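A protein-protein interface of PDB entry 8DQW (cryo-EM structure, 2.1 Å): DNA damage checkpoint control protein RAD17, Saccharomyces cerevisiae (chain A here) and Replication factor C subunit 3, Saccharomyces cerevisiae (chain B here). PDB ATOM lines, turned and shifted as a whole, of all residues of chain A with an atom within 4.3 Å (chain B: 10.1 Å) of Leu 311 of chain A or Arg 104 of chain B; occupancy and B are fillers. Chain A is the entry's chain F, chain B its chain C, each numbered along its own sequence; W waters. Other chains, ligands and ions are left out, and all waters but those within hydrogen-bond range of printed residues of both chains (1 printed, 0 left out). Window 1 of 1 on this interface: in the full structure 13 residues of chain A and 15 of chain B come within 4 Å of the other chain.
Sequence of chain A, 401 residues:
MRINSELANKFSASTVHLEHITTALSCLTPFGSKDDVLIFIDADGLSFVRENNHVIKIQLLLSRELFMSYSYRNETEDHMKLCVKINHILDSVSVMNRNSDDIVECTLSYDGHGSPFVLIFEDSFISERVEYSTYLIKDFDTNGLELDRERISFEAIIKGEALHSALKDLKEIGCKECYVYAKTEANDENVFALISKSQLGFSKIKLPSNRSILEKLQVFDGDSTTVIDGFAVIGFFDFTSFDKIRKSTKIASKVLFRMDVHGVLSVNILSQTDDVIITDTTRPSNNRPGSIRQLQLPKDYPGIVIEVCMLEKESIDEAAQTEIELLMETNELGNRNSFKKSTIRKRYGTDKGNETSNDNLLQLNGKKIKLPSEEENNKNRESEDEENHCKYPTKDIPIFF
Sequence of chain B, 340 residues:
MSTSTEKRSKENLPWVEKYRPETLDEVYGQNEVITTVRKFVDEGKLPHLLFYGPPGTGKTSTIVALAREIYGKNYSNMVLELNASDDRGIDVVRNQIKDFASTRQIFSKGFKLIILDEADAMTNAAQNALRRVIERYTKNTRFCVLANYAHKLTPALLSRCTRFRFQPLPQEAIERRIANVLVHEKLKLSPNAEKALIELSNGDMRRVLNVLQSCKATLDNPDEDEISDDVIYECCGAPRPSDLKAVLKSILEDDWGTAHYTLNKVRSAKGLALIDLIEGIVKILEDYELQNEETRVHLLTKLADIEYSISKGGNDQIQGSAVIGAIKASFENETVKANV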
ATOM      1  N   HIS A  54       7.795  25.728  20.207  1.00  0.00           N
ATOM      2  CA  HIS A  54       6.789  25.292  19.242  1.00  0.00           C
ATOM      3  C   HIS A  54       5.379  25.347  19.821  1.00  0.00           C
ATOM      4  O   HIS A  54       4.450  24.765  19.252  1.00  0.00           O
ATOM      5  CB  HIS A  54       7.085  23.875  18.736  1.00  0.00           C
ATOM      6  CG  HIS A  54       8.376  23.755  17.986  1.00  0.00           C
ATOM      7  ND1 HIS A  54       8.441  23.304  16.685  1.00  0.00           N
ATOM      8  CD2 HIS A  54       9.650  24.029  18.354  1.00  0.00           C
ATOM      9  CE1 HIS A  54       9.700  23.303  16.285  1.00  0.00           C
ATOM     10  NE2 HIS A  54      10.454  23.740  17.278  1.00  0.00           N
ATOM     11  N   VAL A  55       5.199  26.041  20.943  1.00  0.00           N
ATOM     12  CA  VAL A  55       3.912  26.077  21.622  1.00  0.00           C
ATOM     13  C   VAL A  55       3.351  27.482  21.760  1.00  0.00           C
ATOM     14  O   VAL A  55       2.126  27.623  21.915  1.00  0.00           O
ATOM     15  CB  VAL A  55       3.994  25.406  23.010  1.00  0.00           C
ATOM     16  CG1 VAL A  55       4.261  23.912  22.869  1.00  0.00           C
ATOM     17  CG2 VAL A  55       5.053  26.076  23.870  1.00  0.00           C
ATOM     18  N   LEU A 145       1.265  27.852  13.805  1.00  0.00           N
ATOM     19  CA  LEU A 145       0.457  28.082  15.002  1.00  0.00           C
ATOM     20  C   LEU A 145      -0.448  29.279  14.742  1.00  0.00           C
ATOM     21  O   LEU A 145      -0.030  30.430  14.881  1.00  0.00           O
ATOM     22  CB  LEU A 145       1.350  28.305  16.218  1.00  0.00           C
ATOM     23  CG  LEU A 145       0.670  28.391  17.590  1.00  0.00           C
ATOM     24  CD1 LEU A 145      -0.547  27.478  17.687  1.00  0.00           C
ATOM     25  CD2 LEU A 145       1.665  28.064  18.694  1.00  0.00           C
ATOM     26  N   PHE A 237      -4.051  25.944  30.353  1.00  0.00           N
ATOM     27  CA  PHE A 237      -2.760  26.431  29.888  1.00  0.00           C
ATOM     28  C   PHE A 237      -1.737  26.391  31.015  1.00  0.00           C
ATOM     29  O   PHE A 237      -2.080  26.475  32.200  1.00  0.00           O
ATOM     30  CB  PHE A 237      -2.864  27.867  29.349  1.00  0.00           C
ATOM     31  CG  PHE A 237      -3.829  28.020  28.210  1.00  0.00           C
ATOM     32  CD1 PHE A 237      -3.431  27.765  26.907  1.00  0.00           C
ATOM     33  CD2 PHE A 237      -5.134  28.417  28.441  1.00  0.00           C
ATOM     34  CE1 PHE A 237      -4.319  27.903  25.856  1.00  0.00           C
ATOM     35  CE2 PHE A 237      -6.026  28.558  27.394  1.00  0.00           C
ATOM     36  CZ  PHE A 237      -5.616  28.299  26.101  1.00  0.00           C
ATOM     37  N   VAL A 261     -11.640  25.329  18.655  1.00  0.00           N
ATOM     38  CA  VAL A 261     -11.850  23.968  19.140  1.00  0.00           C
ATOM     39  C   VAL A 261     -10.571  23.143  19.114  1.00  0.00           C
ATOM     40  O   VAL A 261     -10.465  22.158  19.855  1.00  0.00           O
ATOM     41  CB  VAL A 261     -12.937  23.253  18.318  1.00  0.00           C
ATOM     42  CG1 VAL A 261     -14.176  24.124  18.197  1.00  0.00           C
ATOM     43  CG2 VAL A 261     -12.408  22.876  16.941  1.00  0.00           C
ATOM     44  N   GLY A 263      -7.840  23.787  20.369  1.00  0.00           N
ATOM     45  CA  GLY A 263      -6.983  24.098  21.494  1.00  0.00           C
ATOM     46  C   GLY A 263      -6.034  25.250  21.264  1.00  0.00           C
ATOM     47  O   GLY A 263      -4.953  25.280  21.861  1.00  0.00           O
ATOM     48  N   VAL A 264      -6.404  26.206  20.415  1.00  0.00           N
ATOM     49  CA  VAL A 264      -5.587  27.381  20.135  1.00  0.00           C
ATOM     50  C   VAL A 264      -6.291  28.605  20.702  1.00  0.00           C
ATOM     51  O   VAL A 264      -7.478  28.835  20.428  1.00  0.00           O
ATOM     52  CB  VAL A 264      -5.323  27.547  18.628  1.00  0.00           C
ATOM     53  CG1 VAL A 264      -4.576  28.847  18.358  1.00  0.00           C
ATOM     54  CG2 VAL A 264      -4.542  26.357  18.089  1.00  0.00           C
ATOM     55  N   MET A 310      -1.265  30.744  21.460  1.00  0.00           N
ATOM     56  CA  MET A 310      -0.743  29.708  22.341  1.00  0.00           C
ATOM     57  C   MET A 310      -1.608  28.458  22.260  1.00  0.00           C
ATOM     58  O   MET A 310      -2.820  28.525  22.032  1.00  0.00           O
ATOM     59  CB  MET A 310      -0.667  30.187  23.800  1.00  0.00           C
ATOM     60  CG  MET A 310      -1.941  30.819  24.326  1.00  0.00           C
ATOM     61  SD  MET A 310      -1.736  31.478  25.993  1.00  0.00           S
ATOM     62  CE  MET A 310      -1.447  33.210  25.640  1.00  0.00           C
ATOM     63  N   LEU A 311      -0.961  27.313  22.452  1.00  0.00           N
ATOM     64  CA  LEU A 311      -1.638  26.027  22.512  1.00  0.00           C
ATOM     65  C   LEU A 311      -1.968  25.676  23.956  1.00  0.00           C
ATOM     66  O   LEU A 311      -1.265  26.073  24.889  1.00  0.00           O
ATOM     67  CB  LEU A 311      -0.768  24.929  21.901  1.00  0.00           C
ATOM     68  CG  LEU A 311      -0.619  24.959  20.379  1.00  0.00           C
ATOM     69  CD1 LEU A 311       0.597  24.153  19.949  1.00  0.00           C
ATOM     70  CD2 LEU A 311      -1.878  24.438  19.703  1.00  0.00           C
ATOM     71  N   GLU A 312      -3.048  24.924  24.133  1.00  0.00           N
ATOM     72  CA  GLU A 312      -3.478  24.481  25.448  1.00  0.00           C
ATOM     73  C   GLU A 312      -2.957  23.072  25.730  1.00  0.00           C
ATOM     74  O   GLU A 312      -2.453  22.378  24.845  1.00  0.00           O
ATOM     75  CB  GLU A 312      -5.008  24.538  25.556  1.00  0.00           C
ATOM     76  CG  GLU A 312      -5.765  23.414  24.861  1.00  0.00           C
ATOM     77  CD  GLU A 312      -7.213  23.335  25.310  1.00  0.00           C
ATOM     78  OE1 GLU A 312      -7.453  22.982  26.484  1.00  0.00           O
ATOM     79  OE2 GLU A 312      -8.112  23.629  24.495  1.00  0.00           O
ATOM     80  N   LYS A 313      -3.082  22.657  26.987  1.00  0.00           N
ATOM     81  CA  LYS A 313      -2.663  21.319  27.377  1.00  0.00           C
ATOM     82  C   LYS A 313      -3.614  20.275  26.796  1.00  0.00           C
ATOM     83  O   LYS A 313      -4.741  20.575  26.396  1.00  0.00           O
ATOM     84  CB  LYS A 313      -2.605  21.187  28.899  1.00  0.00           C
ATOM     85  CG  LYS A 313      -2.022  22.395  29.628  1.00  0.00           C
ATOM     86  CD  LYS A 313      -0.593  22.689  29.195  1.00  0.00           C
ATOM     87  CE  LYS A 313       0.352  21.561  29.575  1.00  0.00           C
ATOM     88  NZ  LYS A 313       1.587  22.058  30.241  1.00  0.00           N
ATOM     89  N   GLU A 314      -3.143  19.025  26.757  1.00  0.00           N
ATOM     90  CA  GLU A 314      -3.918  17.964  26.116  1.00  0.00           C
ATOM     91  C   GLU A 314      -5.270  17.784  26.793  1.00  0.00           C
ATOM     92  O   GLU A 314      -6.314  17.774  26.131  1.00  0.00           O
ATOM     93  CB  GLU A 314      -3.152  16.641  26.149  1.00  0.00           C
ATOM     94  CG  GLU A 314      -2.095  16.478  25.066  1.00  0.00           C
ATOM     95  CD  GLU A 314      -0.692  16.670  25.595  1.00  0.00           C
ATOM     96  OE1 GLU A 314      -0.491  16.530  26.819  1.00  0.00           O
ATOM     97  OE2 GLU A 314       0.213  16.962  24.789  1.00  0.00           O
ATOM     98  N   ASN B  77       6.277  21.481  11.662  1.00  0.00           N
ATOM     99  CA  ASN B  77       5.448  22.212  12.613  1.00  0.00           C
ATOM    100  C   ASN B  77       5.017  21.370  13.807  1.00  0.00           C
ATOM    101  O   ASN B  77       4.643  21.933  14.843  1.00  0.00           O
ATOM    102  CB  ASN B  77       4.206  22.761  11.906  1.00  0.00           C
ATOM    103  CG  ASN B  77       4.552  23.649  10.731  1.00  0.00           C
ATOM    104  OD1 ASN B  77       5.380  24.553  10.844  1.00  0.00           O
ATOM    105  ND2 ASN B  77       3.921  23.395   9.590  1.00  0.00           N
ATOM    106  N   MET B  78       5.061  20.040  13.696  1.00  0.00           N
ATOM    107  CA  MET B  78       4.635  19.154  14.775  1.00  0.00           C
ATOM    108  C   MET B  78       5.673  18.080  15.084  1.00  0.00           C
ATOM    109  O   MET B  78       5.331  17.034  15.644  1.00  0.00           O
ATOM    110  CB  MET B  78       3.294  18.505  14.434  1.00  0.00           C
ATOM    111  CG  MET B  78       3.255  17.851  13.061  1.00  0.00           C
ATOM    112  SD  MET B  78       2.757  18.972  11.737  1.00  0.00           S
ATOM    113  CE  MET B  78       1.183  19.579  12.342  1.00  0.00           C
ATOM    114  N   VAL B  79       6.932  18.315  14.729  1.00  0.00           N
ATOM    115  CA  VAL B  79       8.039  17.431  15.070  1.00  0.00           C
ATOM    116  C   VAL B  79       9.078  18.259  15.815  1.00  0.00           C
ATOM    117  O   VAL B  79       9.476  19.329  15.342  1.00  0.00           O
ATOM    118  CB  VAL B  79       8.652  16.776  13.818  1.00  0.00           C
ATOM    119  CG1 VAL B  79       9.938  16.045  14.170  1.00  0.00           C
ATOM    120  CG2 VAL B  79       7.652  15.830  13.167  1.00  0.00           C
ATOM    121  N   LYS B  98       9.174  18.626  27.949  1.00  0.00           N
ATOM    122  CA  LYS B  98       7.956  18.411  28.724  1.00  0.00           C
ATOM    123  C   LYS B  98       6.799  19.238  28.175  1.00  0.00           C
ATOM    124  O   LYS B  98       5.693  18.722  27.980  1.00  0.00           O
ATOM    125  CB  LYS B  98       8.219  18.757  30.190  1.00  0.00           C
ATOM    126  CG  LYS B  98       7.046  18.531  31.124  1.00  0.00           C
ATOM    127  CD  LYS B  98       7.495  17.869  32.419  1.00  0.00           C
ATOM    128  CE  LYS B  98       6.325  17.647  33.357  1.00  0.00           C
ATOM    129  NZ  LYS B  98       6.707  16.867  34.570  1.00  0.00           N
ATOM    130  N   ASP B  99       7.033  20.529  27.914  1.00  0.00           N
ATOM    131  CA  ASP B  99       5.961  21.382  27.415  1.00  0.00           C
ATOM    132  C   ASP B  99       5.523  20.967  26.017  1.00  0.00           C
ATOM    133  O   ASP B  99       4.324  20.978  25.712  1.00  0.00           O
ATOM    134  CB  ASP B  99       6.397  22.847  27.428  1.00  0.00           C
ATOM    135  CG  ASP B  99       6.750  23.341  28.819  1.00  0.00           C
ATOM    136  OD1 ASP B  99       7.748  24.081  28.957  1.00  0.00           O
ATOM    137  OD2 ASP B  99       6.030  22.988  29.778  1.00  0.00           O
ATOM    138  N   PHE B 100       6.469  20.602  25.148  1.00  0.00           N
ATOM    139  CA  PHE B 100       6.083  20.158  23.813  1.00  0.00           C
ATOM    140  C   PHE B 100       5.252  18.884  23.875  1.00  0.00           C
ATOM    141  O   PHE B 100       4.239  18.759  23.177  1.00  0.00           O
ATOM    142  CB  PHE B 100       7.317  19.934  22.940  1.00  0.00           C
ATOM    143  CG  PHE B 100       6.989  19.509  21.535  1.00  0.00           C
ATOM    144  CD1 PHE B 100       6.544  20.433  20.604  1.00  0.00           C
ATOM    145  CD2 PHE B 100       7.103  18.183  21.153  1.00  0.00           C
ATOM    146  CE1 PHE B 100       6.234  20.045  19.312  1.00  0.00           C
ATOM    147  CE2 PHE B 100       6.795  17.789  19.863  1.00  0.00           C
ATOM    148  CZ  PHE B 100       6.358  18.722  18.942  1.00  0.00           C
ATOM    149  N   ALA B 101       5.660  17.926  24.711  1.00  0.00           N
ATOM    150  CA  ALA B 101       4.958  16.651  24.784  1.00  0.00           C
ATOM    151  C   ALA B 101       3.615  16.763  25.492  1.00  0.00           C
ATOM    152  O   ALA B 101       2.769  15.878  25.324  1.00  0.00           O
ATOM    153  CB  ALA B 101       5.826  15.614  25.498  1.00  0.00           C
ATOM    154  N   SER B 102       3.401  17.820  26.274  1.00  0.00           N
ATOM    155  CA  SER B 102       2.194  17.974  27.072  1.00  0.00           C
ATOM    156  C   SER B 102       1.201  18.963  26.469  1.00  0.00           C
ATOM    157  O   SER B 102       0.248  19.354  27.149  1.00  0.00           O
ATOM    158  CB  SER B 102       2.559  18.409  28.492  1.00  0.00           C
ATOM    159  OG  SER B 102       3.125  19.708  28.499  1.00  0.00           O
ATOM    160  N   THR B 103       1.391  19.363  25.214  1.00  0.00           N
ATOM    161  CA  THR B 103       0.515  20.316  24.547  1.00  0.00           C
ATOM    162  C   THR B 103      -0.141  19.666  23.334  1.00  0.00           C
ATOM    163  O   THR B 103       0.362  18.686  22.778  1.00  0.00           O
ATOM    164  CB  THR B 103       1.282  21.576  24.116  1.00  0.00           C
ATOM    165  OG1 THR B 103       2.536  21.203  23.531  1.00  0.00           O
ATOM    166  CG2 THR B 103       1.525  22.490  25.309  1.00  0.00           C
ATOM    167  N   ARG B 104      -1.276  20.230  22.928  1.00  0.00           N
ATOM    168  CA  ARG B 104      -2.061  19.660  21.843  1.00  0.00           C
ATOM    169  C   ARG B 104      -1.338  19.802  20.507  1.00  0.00           C
ATOM    170  O   ARG B 104      -0.405  20.593  20.348  1.00  0.00           O
ATOM    171  CB  ARG B 104      -3.429  20.337  21.751  1.00  0.00           C
ATOM    172  CG  ARG B 104      -4.254  20.252  23.015  1.00  0.00           C
ATOM    173  CD  ARG B 104      -5.679  19.824  22.711  1.00  0.00           C
ATOM    174  NE  ARG B 104      -6.517  19.814  23.905  1.00  0.00           N
ATOM    175  CZ  ARG B 104      -7.843  19.852  23.891  1.00  0.00           C
ATOM    176  NH1 ARG B 104      -8.523  19.902  22.757  1.00  0.00           N
ATOM    177  NH2 ARG B 104      -8.503  19.839  25.045  1.00  0.00           N
ATOM    178  N   GLN B 105      -1.793  19.015  19.535  1.00  0.00           N
ATOM    179  CA  GLN B 105      -1.286  19.118  18.177  1.00  0.00           C
ATOM    180  C   GLN B 105      -1.759  20.418  17.532  1.00  0.00           C
ATOM    181  O   GLN B 105      -2.713  21.058  17.982  1.00  0.00           O
ATOM    182  CB  GLN B 105      -1.744  17.925  17.340  1.00  0.00           C
ATOM    183  CG  GLN B 105      -0.669  16.878  17.113  1.00  0.00           C
ATOM    184  CD  GLN B 105       0.377  17.318  16.109  1.00  0.00           C
ATOM    185  OE1 GLN B 105       0.758  18.487  16.059  1.00  0.00           O
ATOM    186  NE2 GLN B 105       0.852  16.376  15.302  1.00  0.00           N
ATOM    187  N   ILE B 106      -1.072  20.806  16.455  1.00  0.00           N
ATOM    188  CA  ILE B 106      -1.359  22.086  15.812  1.00  0.00           C
ATOM    189  C   ILE B 106      -2.796  22.116  15.307  1.00  0.00           C
ATOM    190  O   ILE B 106      -3.525  23.093  15.517  1.00  0.00           O
ATOM    191  CB  ILE B 106      -0.357  22.346  14.670  1.00  0.00           C
ATOM    192  CG1 ILE B 106       1.072  22.532  15.204  1.00  0.00           C
ATOM    193  CG2 ILE B 106      -0.771  23.576  13.872  1.00  0.00           C
ATOM    194  CD1 ILE B 106       1.182  23.174  16.574  1.00  0.00           C
ATOM    195  N   PHE B 107      -3.223  21.051  14.632  1.00  0.00           N
ATOM    196  CA  PHE B 107      -4.567  20.952  14.072  1.00  0.00           C
ATOM    197  C   PHE B 107      -5.176  19.592  14.377  1.00  0.00           C
ATOM    198  O   PHE B 107      -5.847  18.987  13.535  1.00  0.00           O
ATOM    199  CB  PHE B 107      -4.552  21.198  12.565  1.00  0.00           C
ATOM    200  CG  PHE B 107      -4.051  22.558  12.172  1.00  0.00           C
ATOM    201  CD1 PHE B 107      -4.523  23.697  12.804  1.00  0.00           C
ATOM    202  CD2 PHE B 107      -3.109  22.699  11.165  1.00  0.00           C
ATOM    203  CE1 PHE B 107      -4.062  24.949  12.442  1.00  0.00           C
ATOM    204  CE2 PHE B 107      -2.646  23.948  10.800  1.00  0.00           C
ATOM    205  CZ  PHE B 107      -3.124  25.074  11.438  1.00  0.00           C
ATOM    206  N   SER B 108      -4.956  19.090  15.592  1.00  0.00           N
ATOM    207  CA  SER B 108      -5.456  17.775  15.992  1.00  0.00           C
ATOM    208  C   SER B 108      -4.982  16.695  15.021  1.00  0.00           C
ATOM    209  O   SER B 108      -5.724  15.773  14.677  1.00  0.00           O
ATOM    210  CB  SER B 108      -6.983  17.778  16.096  1.00  0.00           C
ATOM    211  OG  SER B 108      -7.435  16.776  16.991  1.00  0.00           O
ATOM    212  N   LYS B 109      -3.730  16.811  14.577  1.00  0.00           N
ATOM    213  CA  LYS B 109      -3.154  15.868  13.618  1.00  0.00           C
ATOM    214  C   LYS B 109      -2.544  14.684  14.369  1.00  0.00           C
ATOM    215  O   LYS B 109      -1.333  14.452  14.374  1.00  0.00           O
ATOM    216  CB  LYS B 109      -2.119  16.566  12.744  1.00  0.00           C
ATOM    217  CG  LYS B 109      -2.577  17.895  12.154  1.00  0.00           C
ATOM    218  CD  LYS B 109      -3.654  17.704  11.095  1.00  0.00           C
ATOM    219  CE  LYS B 109      -3.046  17.441   9.726  1.00  0.00           C
ATOM    220  NZ  LYS B 109      -4.061  17.505   8.638  1.00  0.00           N
ATOM    221  N   GLY B 110      -3.423  13.920  15.010  1.00  0.00           N
ATOM    222  CA  GLY B 110      -2.978  12.737  15.730  1.00  0.00           C
ATOM    223  C   GLY B 110      -1.981  13.091  16.816  1.00  0.00           C
ATOM    224  O   GLY B 110      -2.174  14.038  17.586  1.00  0.00           O
ATOM    225  N   PHE B 111      -0.897  12.325  16.883  1.00  0.00           N
ATOM    226  CA  PHE B 111       0.110  12.478  17.922  1.00  0.00           C
ATOM    227  C   PHE B 111       1.296  13.290  17.415  1.00  0.00           C
ATOM    228  O   PHE B 111       1.497  13.463  16.211  1.00  0.00           O
ATOM    229  CB  PHE B 111       0.589  11.109  18.421  1.00  0.00           C
ATOM    230  CG  PHE B 111       1.116  10.213  17.335  1.00  0.00           C
ATOM    231  CD1 PHE B 111       2.362  10.436  16.772  1.00  0.00           C
ATOM    232  CD2 PHE B 111       0.366   9.141  16.881  1.00  0.00           C
ATOM    233  CE1 PHE B 111       2.845   9.614  15.773  1.00  0.00           C
ATOM    234  CE2 PHE B 111       0.845   8.313  15.885  1.00  0.00           C
ATOM    235  CZ  PHE B 111       2.086   8.550  15.331  1.00  0.00           C
ATOM    236  N   LYS B 112       2.084  13.787  18.361  1.00  0.00           N
ATOM    237  CA  LYS B 112       3.297  14.538  18.077  1.00  0.00           C
ATOM    238  C   LYS B 112       4.507  13.612  18.143  1.00  0.00           C
ATOM    239  O   LYS B 112       4.463  12.537  18.747  1.00  0.00           O
ATOM    240  CB  LYS B 112       3.458  15.698  19.065  1.00  0.00           C
ATOM    241  CG  LYS B 112       2.231  16.594  19.163  1.00  0.00           C
ATOM    242  CD  LYS B 112       2.290  17.535  20.358  1.00  0.00           C
ATOM    243  CE  LYS B 112       2.650  18.951  19.936  1.00  0.00           C
ATOM    244  NZ  LYS B 112       3.330  19.713  21.017  1.00  0.00           N
ATOM    245  N   LEU B 113       5.595  14.042  17.509  1.00  0.00           N
ATOM    246  CA  LEU B 113       6.814  13.250  17.414  1.00  0.00           C
ATOM    247  C   LEU B 113       7.991  14.050  17.954  1.00  0.00           C
ATOM    248  O   LEU B 113       8.186  15.212  17.578  1.00  0.00           O
ATOM    249  CB  LEU B 113       7.078  12.824  15.966  1.00  0.00           C
ATOM    250  CG  LEU B 113       8.323  11.969  15.722  1.00  0.00           C
ATOM    251  CD1 LEU B 113       8.212  10.634  16.441  1.00  0.00           C
ATOM    252  CD2 LEU B 113       8.541  11.760  14.231  1.00  0.00           C
ATOM    253  N   TYR B 137       2.860  10.708  28.629  1.00  0.00           N
ATOM    254  CA  TYR B 137       2.325  11.365  27.441  1.00  0.00           C
ATOM    255  C   TYR B 137       2.373  10.471  26.207  1.00  0.00           C
ATOM    256  O   TYR B 137       2.449  10.974  25.081  1.00  0.00           O
ATOM    257  CB  TYR B 137       3.084  12.667  27.186  1.00  0.00           C
ATOM    258  CG  TYR B 137       2.984  13.652  28.327  1.00  0.00           C
ATOM    259  CD1 TYR B 137       1.766  14.226  28.664  1.00  0.00           C
ATOM    260  CD2 TYR B 137       4.101  13.997  29.076  1.00  0.00           C
ATOM    261  CE1 TYR B 137       1.664  15.123  29.705  1.00  0.00           C
ATOM    262  CE2 TYR B 137       4.008  14.893  30.124  1.00  0.00           C
ATOM    263  CZ  TYR B 137       2.786  15.453  30.433  1.00  0.00           C
ATOM    264  OH  TYR B 137       2.679  16.346  31.473  1.00  0.00           O
ATOM    265  N   LYS B 139       0.001   8.729  24.923  1.00  0.00           N
ATOM    266  CA  LYS B 139      -1.205   8.878  24.117  1.00  0.00           C
ATOM    267  C   LYS B 139      -1.032   9.965  23.063  1.00  0.00           C
ATOM    268  O   LYS B 139      -1.440   9.791  21.909  1.00  0.00           O
ATOM    269  CB  LYS B 139      -2.402   9.197  25.014  1.00  0.00           C
ATOM    270  CG  LYS B 139      -3.739   9.297  24.257  1.00  0.00           C
ATOM    271  CD  LYS B 139      -4.809  10.191  24.913  1.00  0.00           C
ATOM    272  CE  LYS B 139      -4.262  11.449  25.587  1.00  0.00           C
ATOM    273  NZ  LYS B 139      -3.601  12.358  24.610  1.00  0.00           N
ATOM    274  N   ASN B 140      -0.427  11.092  23.437  1.00  0.00           N
ATOM    275  CA  ASN B 140      -0.335  12.240  22.549  1.00  0.00           C
ATOM    276  C   ASN B 140       0.997  12.351  21.820  1.00  0.00           C
ATOM    277  O   ASN B 140       1.061  13.029  20.789  1.00  0.00           O
ATOM    278  CB  ASN B 140      -0.568  13.538  23.337  1.00  0.00           C
ATOM    279  CG  ASN B 140      -0.840  14.730  22.431  1.00  0.00           C
ATOM    280  OD1 ASN B 140      -0.363  15.832  22.685  1.00  0.00           O
ATOM    281  ND2 ASN B 140      -1.638  14.523  21.389  1.00  0.00           N
ATOM    282  N   THR B 141       2.057  11.718  22.321  1.00  0.00           N
ATOM    283  CA  THR B 141       3.392  11.921  21.781  1.00  0.00           C
ATOM    284  C   THR B 141       4.128  10.592  21.686  1.00  0.00           C
ATOM    285  O   THR B 141       3.894   9.676  22.478  1.00  0.00           O
ATOM    286  CB  THR B 141       4.198  12.900  22.652  1.00  0.00           C
ATOM    287  OG1 THR B 141       3.443  14.101  22.848  1.00  0.00           O
ATOM    288  CG2 THR B 141       5.527  13.241  21.992  1.00  0.00           C
HETATM  289  O   HOH W   1       3.516  22.043  19.226  1.00  0.00           O
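The backbone carbonyl oxygen (O) of Phe 100 of chain B sits at hydrogen-bond distance from the side-chain amino group (NZ) of Lys 112 of chain B (2.5 Å).
The backbone NH (N) of Lys 112 of chain B sits at hydrogen-bond distance from the backbone carbonyl oxygen (O) of Asn 140 of chain B, 2.7 Å away.
No residue of chain B comes within 4 Å of Gly 263 of chain A.
Of chain B, only Arg 104, Gln 105 and Ile 106 come within 4 Å of Leu 311 of chain A.
Of chain B, only Thr 103 and Arg 104 come within 4 Å of Glu 312 of chain A.
Asp 99 of chain B touches none of the printed residues of chain A.
Of the printed residues of chain A, Ala 101 of chain B touches Glu 314.
Arg 104 of chain B touches just these residues of chain A: Leu 311, Glu 312, Lys 313 and Glu 314.
Of the printed residues of chain A, Gln 105 of chain B touches Leu 311.
Phe 107 of chain B touches none of the printed residues of chain A.
CB of His 54 of chain A touches CD1 of Phe 100 of chain B, 3.95 Å away.
OG1 of Thr 103 of chain B touches CG1 of Val 55 of chain A, at 3.3 Å.
CD1 of Leu 311 of chain A touches O of Arg 104 of chain B, at 3.7 Å.
CD2 of Leu 311 of chain A touches O of Gln 105 of chain B, 3.9 Å away.
Glu 312 of chain A touches Thr 103 of chain B (O to CA, 3.6 Å).
Glu 314 of chain A touches Tyr 137 of chain B (OE1 to CD1, 3.7 Å).
Printed residues of chain B that touch a printed residue of chain A: Phe 100, Ala 101, Ser 102, Thr 103, Arg 104, Gln 105, Ile 106, Tyr 137 and Asn 140.
Of the 12 printed residues of chain A, 6 touch a printed residue of chain B.
Printed residues of chain A that touch a printed residue of chain B: His 54, Val 55, Leu 311, Glu 312, Lys 313 and Glu 314.
Hydrophobic or aromatic side chains of chain A that line the printed part of chain B: His 54, Val 55 and Leu 311.
Along chain A the printed residues that touch a printed residue of chain B span positions 54 to 314.
Among the printed residues, 15 pairs touch across the chains.
The backbone carbonyl oxygen (O) of Ala 101 of chain B sits close to the side-chain carboxylate (OE2) of Glu 314 of chain A (2.8 Å).
NZ of Lys 313 of chain A is in hydrogen-bond range of OG of Ser 102 of chain B, 3.3 Å away.
OD1 of Asn 140 of chain B lies close to OE2 of Glu 314 of chain A, 2.5 Å away.
The side-chain carboxylate of Glu 314 of chain A lies within hydrogen-bond range of the backbone NH of Thr 103 of chain B (2.7 Å).
NE of Arg 104 of chain B lies within hydrogen-bond range of O of Lys 313 of chain A.
The guanidinium group of Arg 104 of chain B lies within hydrogen-bond range of the backbone carbonyl oxygen of Glu 314 of chain A, 3.0 Å away.
The guanidinium group (NH2) of Arg 104 of chain B lies within salt-bridge range of the side-chain carboxylate (OE1) of Glu 312 of chain A, 3.6 Å away.
O of Ser 102 of chain B lies close to N of Glu 314 of chain A (3.4 Å).
Water W1 lies within hydrogen-bond range of O of His 54 of chain A and NZ of Lys 112 of chain B.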
